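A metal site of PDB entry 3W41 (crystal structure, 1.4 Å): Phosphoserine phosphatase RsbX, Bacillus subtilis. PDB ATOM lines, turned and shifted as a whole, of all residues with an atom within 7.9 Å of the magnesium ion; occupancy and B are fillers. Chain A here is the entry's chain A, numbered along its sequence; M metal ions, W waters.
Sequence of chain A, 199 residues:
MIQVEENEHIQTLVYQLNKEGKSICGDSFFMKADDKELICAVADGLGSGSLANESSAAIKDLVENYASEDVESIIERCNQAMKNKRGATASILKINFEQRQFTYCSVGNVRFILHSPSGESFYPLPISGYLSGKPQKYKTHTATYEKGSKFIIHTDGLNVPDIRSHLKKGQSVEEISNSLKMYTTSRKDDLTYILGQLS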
ATOM      1  N   LYS A  22       4.566 -23.707  20.545  1.00  0.00           N
ATOM      2  CA  LYS A  22       3.696 -24.633  19.781  1.00  0.00           C
ATOM      3  C   LYS A  22       3.288 -23.944  18.472  1.00  0.00           C
ATOM      4  O   LYS A  22       2.669 -22.874  18.499  1.00  0.00           O
ATOM      5  CB  LYS A  22       2.479 -24.972  20.654  1.00  0.00           C
ATOM      6  CG  LYS A  22       1.566 -26.135  20.196  1.00  0.00           C
ATOM      7  CD  LYS A  22       0.362 -26.291  21.146  1.00  0.00           C
ATOM      8  CE  LYS A  22      -0.600 -27.368  20.634  1.00  0.00           C
ATOM      9  NZ  LYS A  22      -1.809 -27.533  21.504  1.00  0.00           N
ATOM     10  N   GLY A  26      -4.433 -25.982  18.496  1.00  0.00           N
ATOM     11  CA  GLY A  26      -5.502 -26.986  18.542  1.00  0.00           C
ATOM     12  C   GLY A  26      -6.898 -26.401  18.714  1.00  0.00           C
ATOM     13  O   GLY A  26      -7.885 -27.139  18.608  1.00  0.00           O
ATOM     14  N   ASP A  27      -6.981 -25.104  18.978  1.00  0.00           N
ATOM     15  CA  ASP A  27      -8.267 -24.411  19.129  1.00  0.00           C
ATOM     16  C   ASP A  27      -8.696 -23.809  17.796  1.00  0.00           C
ATOM     17  O   ASP A  27      -7.834 -23.483  16.953  1.00  0.00           O
ATOM     18  CB  ASP A  27      -8.136 -23.201  20.080  1.00  0.00           C
ATOM     19  CG  ASP A  27      -7.956 -23.537  21.574  1.00  0.00           C
ATOM     20  OD1 ASP A  27      -7.924 -24.711  21.997  1.00  0.00           O
ATOM     21  OD2 ASP A  27      -7.834 -22.524  22.377  1.00  0.00           O
ATOM     22  N   ALA A  43     -13.890 -24.050  19.590  1.00  0.00           N
ATOM     23  CA  ALA A  43     -13.676 -25.486  19.725  1.00  0.00           C
ATOM     24  C   ALA A  43     -12.238 -25.763  20.075  1.00  0.00           C
ATOM     25  O   ALA A  43     -11.339 -25.006  19.720  1.00  0.00           O
ATOM     26  CB  ALA A  43     -14.054 -26.204  18.406  1.00  0.00           C
ATOM     27  N   ASP A  44     -12.024 -26.860  20.799  1.00  0.00           N
ATOM     28  CA  ASP A  44     -10.698 -27.286  21.249  1.00  0.00           C
ATOM     29  C   ASP A  44     -10.543 -28.762  20.884  1.00  0.00           C
ATOM     30  O   ASP A  44     -11.218 -29.601  21.440  1.00  0.00           O
ATOM     31  CB  ASP A  44     -10.588 -27.007  22.773  1.00  0.00           C
ATOM     32  CG  ASP A  44      -9.265 -27.406  23.357  1.00  0.00           C
ATOM     33  OD1 ASP A  44      -8.457 -28.057  22.672  1.00  0.00           O
ATOM     34  OD2 ASP A  44      -9.012 -27.097  24.560  1.00  0.00           O
ATOM     35  N   GLY A  45      -9.720 -29.052  19.889  1.00  0.00           N
ATOM     36  CA  GLY A  45      -9.507 -30.421  19.438  1.00  0.00           C
ATOM     37  C   GLY A  45      -8.790 -31.298  20.450  1.00  0.00           C
ATOM     38  O   GLY A  45      -7.930 -30.819  21.229  1.00  0.00           O
ATOM     39  N   GLY A  47      -6.329 -34.359  21.751  1.00  0.00           N
ATOM     40  CA  GLY A  47      -4.969 -34.704  21.401  1.00  0.00           C
ATOM     41  C   GLY A  47      -4.132 -33.517  21.066  1.00  0.00           C
ATOM     42  O   GLY A  47      -4.387 -32.415  21.498  1.00  0.00           O
ATOM     43  N   THR A  89     -13.955 -30.518  22.079  1.00  0.00           N
ATOM     44  CA  THR A  89     -14.951 -29.867  22.885  1.00  0.00           C
ATOM     45  C   THR A  89     -15.356 -28.582  22.144  1.00  0.00           C
ATOM     46  O   THR A  89     -14.557 -28.018  21.392  1.00  0.00           O
ATOM     47  CB  THR A  89     -14.427 -29.565  24.310  1.00  0.00           C
ATOM     48  OG1 THR A  89     -13.266 -28.719  24.229  1.00  0.00           O
ATOM     49  CG2 THR A  89     -14.071 -30.907  25.016  1.00  0.00           C
ATOM     50  N   ASN A 109     -15.697 -28.763  27.651  1.00  0.00           N
ATOM     51  CA  ASN A 109     -15.194 -27.800  28.624  1.00  0.00           C
ATOM     52  C   ASN A 109     -14.926 -26.384  28.105  1.00  0.00           C
ATOM     53  O   ASN A 109     -14.175 -25.623  28.722  1.00  0.00           O
ATOM     54  CB  ASN A 109     -13.915 -28.369  29.296  1.00  0.00           C
ATOM     55  CG  ASN A 109     -12.719 -28.416  28.337  1.00  0.00           C
ATOM     56  OD1 ASN A 109     -12.856 -28.259  27.112  1.00  0.00           O
ATOM     57  ND2 ASN A 109     -11.535 -28.659  28.883  1.00  0.00           N
ATOM     58  N   VAL A 110     -15.514 -26.020  26.963  1.00  0.00           N
ATOM     59  CA  VAL A 110     -15.462 -24.633  26.493  1.00  0.00           C
ATOM     60  C   VAL A 110     -16.547 -23.908  27.290  1.00  0.00           C
ATOM     61  O   VAL A 110     -17.681 -24.378  27.361  1.00  0.00           O
ATOM     62  CB  VAL A 110     -15.654 -24.540  24.977  1.00  0.00           C
ATOM     63  CG1 VAL A 110     -15.570 -23.071  24.502  1.00  0.00           C
ATOM     64  CG2 VAL A 110     -14.543 -25.340  24.255  1.00  0.00           C
ATOM     65  N   THR A 155     -11.794 -21.187  25.792  1.00  0.00           N
ATOM     66  CA  THR A 155     -11.265 -22.522  25.987  1.00  0.00           C
ATOM     67  C   THR A 155     -10.512 -22.679  27.308  1.00  0.00           C
ATOM     68  O   THR A 155     -10.265 -21.701  28.032  1.00  0.00           O
ATOM     69  CB  THR A 155     -10.339 -22.941  24.839  1.00  0.00           C
ATOM     70  OG1 THR A 155      -9.197 -22.074  24.805  1.00  0.00           O
ATOM     71  CG2 THR A 155     -11.013 -22.906  23.471  1.00  0.00           C
ATOM     72  N   ASP A 156     -10.174 -23.926  27.617  1.00  0.00           N
ATOM     73  CA  ASP A 156      -9.634 -24.250  28.921  1.00  0.00           C
ATOM     74  C   ASP A 156      -8.210 -23.729  29.146  1.00  0.00           C
ATOM     75  O   ASP A 156      -7.720 -23.768  30.284  1.00  0.00           O
ATOM     76  CB  ASP A 156      -9.734 -25.770  29.157  1.00  0.00           C
ATOM     77  CG  ASP A 156      -8.907 -26.569  28.179  1.00  0.00           C
ATOM     78  OD1 ASP A 156      -8.275 -26.029  27.250  1.00  0.00           O
ATOM     79  OD2 ASP A 156      -8.885 -27.819  28.320  1.00  0.00           O
ATOM     80  N   GLY A 157      -7.549 -23.148  28.137  1.00  0.00           N
ATOM     81  CA  GLY A 157      -6.237 -22.548  28.361  1.00  0.00           C
ATOM     82  C   GLY A 157      -6.303 -21.262  29.157  1.00  0.00           C
ATOM     83  O   GLY A 157      -5.297 -20.848  29.722  1.00  0.00           O
ATOM     84  N   LEU A 158      -7.484 -20.640  29.214  1.00  0.00           N
ATOM     85  CA  LEU A 158      -7.694 -19.449  30.043  1.00  0.00           C
ATOM     86  C   LEU A 158      -8.096 -19.863  31.472  1.00  0.00           C
ATOM     87  O   LEU A 158      -9.189 -20.363  31.690  1.00  0.00           O
ATOM     88  CB  LEU A 158      -8.722 -18.538  29.383  1.00  0.00           C
ATOM     89  CG  LEU A 158      -9.038 -17.273  30.190  1.00  0.00           C
ATOM     90  CD1 LEU A 158      -7.843 -16.305  30.179  1.00  0.00           C
ATOM     91  CD2 LEU A 158     -10.310 -16.612  29.632  1.00  0.00           C
ATOM     92  N   LYS A 188      -0.699 -22.638  29.929  1.00  0.00           N
ATOM     93  CA  LYS A 188       0.073 -23.857  29.700  1.00  0.00           C
ATOM     94  C   LYS A 188      -0.569 -24.659  28.549  1.00  0.00           C
ATOM     95  O   LYS A 188      -0.342 -25.863  28.366  1.00  0.00           O
ATOM     96  CB  LYS A 188       0.137 -24.693  30.978  1.00  0.00           C
ATOM     97  CG  LYS A 188       0.936 -24.011  32.091  1.00  0.00           C
ATOM     98  CD  LYS A 188       1.102 -24.874  33.334  1.00  0.00           C
ATOM     99  CE  LYS A 188       1.967 -26.128  33.090  1.00  0.00           C
ATOM    100  NZ  LYS A 188       1.150 -27.362  32.823  1.00  0.00           N
ATOM    101  N   ASP A 189      -1.325 -23.941  27.741  1.00  0.00           N
ATOM    102  CA  ASP A 189      -2.139 -24.531  26.676  1.00  0.00           C
ATOM    103  C   ASP A 189      -2.465 -23.416  25.700  1.00  0.00           C
ATOM    104  O   ASP A 189      -2.298 -22.236  26.011  1.00  0.00           O
ATOM    105  CB  ASP A 189      -3.421 -25.099  27.294  1.00  0.00           C
ATOM    106  CG  ASP A 189      -4.276 -25.895  26.308  1.00  0.00           C
ATOM    107  OD1 ASP A 189      -3.786 -26.338  25.254  1.00  0.00           O
ATOM    108  OD2 ASP A 189      -5.458 -26.067  26.643  1.00  0.00           O
ATOM    109  N   ASP A 190      -2.916 -23.782  24.511  1.00  0.00           N
ATOM    110  CA  ASP A 190      -3.584 -22.833  23.634  1.00  0.00           C
ATOM    111  C   ASP A 190      -4.739 -22.164  24.367  1.00  0.00           C
ATOM    112  O   ASP A 190      -5.412 -22.764  25.216  1.00  0.00           O
ATOM    113  CB  ASP A 190      -4.181 -23.553  22.438  1.00  0.00           C
ATOM    114  CG  ASP A 190      -3.169 -24.305  21.650  1.00  0.00           C
ATOM    115  OD1 ASP A 190      -2.013 -23.853  21.509  1.00  0.00           O
ATOM    116  OD2 ASP A 190      -3.516 -25.376  21.131  1.00  0.00           O
ATOM    117  N   LEU A 191      -4.979 -20.908  24.032  1.00  0.00           N
ATOM    118  CA  LEU A 191      -5.968 -20.120  24.735  1.00  0.00           C
ATOM    119  C   LEU A 191      -6.729 -19.332  23.693  1.00  0.00           C
ATOM    120  O   LEU A 191      -6.114 -18.627  22.881  1.00  0.00           O
ATOM    121  CB  LEU A 191      -5.237 -19.175  25.707  1.00  0.00           C
ATOM    122  CG  LEU A 191      -5.990 -18.267  26.674  1.00  0.00           C
ATOM    123  CD1 LEU A 191      -5.053 -17.869  27.794  1.00  0.00           C
ATOM    124  CD2 LEU A 191      -6.552 -17.059  25.968  1.00  0.00           C
ATOM    125  N   THR A 192      -8.051 -19.460  23.691  1.00  0.00           N
ATOM    126  CA  THR A 192      -8.912 -18.696  22.788  1.00  0.00           C
ATOM    127  C   THR A 192     -10.092 -18.145  23.570  1.00  0.00           C
ATOM    128  O   THR A 192     -10.672 -18.857  24.383  1.00  0.00           O
ATOM    129  CB  THR A 192      -9.479 -19.597  21.687  1.00  0.00           C
ATOM    130  OG1 THR A 192      -8.395 -20.212  20.998  1.00  0.00           O
ATOM    131  CG2 THR A 192     -10.357 -18.864  20.721  1.00  0.00           C
HETATM  132 MG    MG M   1      -7.226 -26.692  25.589  1.00  0.00          MG
HETATM  133  O   HOH W   1      -7.187 -24.803  24.693  1.00  0.00           O
HETATM  134  O   HOH W   2      -5.918 -27.485  24.146  1.00  0.00           O
HETATM  135  O   HOH W   3      -7.137 -28.564  26.506  1.00  0.00           O
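The side-chain carboxylate (OD2) of Asp 156 is in hydrogen-bond range of the side-chain amide nitrogen (ND2) of Asn 109.
The backbone carbonyl oxygen (O) of Thr 89 is in hydrogen-bond range of the backbone NH (N) of Asp 44 (2.8 Å).
OD1 of Asp 156 binds the magnesium ion (2.1 Å).
Water W3 binds the magnesium ion.
The magnesium ion is bound by water W1 (2.1 Å).
OD2 of Asp 44 binds the magnesium ion (2.1 Å).
The magnesium ion is bound by water W2 (2.1 Å).
OD2 of Asp 189 is bound to the magnesium ion.
The magnesium ion has six donor atoms within binding distance.
Water W1 lies within hydrogen-bond range of the backbone carbonyl oxygen (O) of Asp 190 (2.8 Å), the side-chain carboxylate (OD1) of Asp 27 (2.8 Å) and the side-chain hydroxyl (OG1) of Thr 155 (3.4 Å).
Water W2 lies within hydrogen-bond range of the side-chain carboxylate of Asp 189 (2.7 Å) and the side-chain carboxylate of Asp 44 (3.0 Å).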
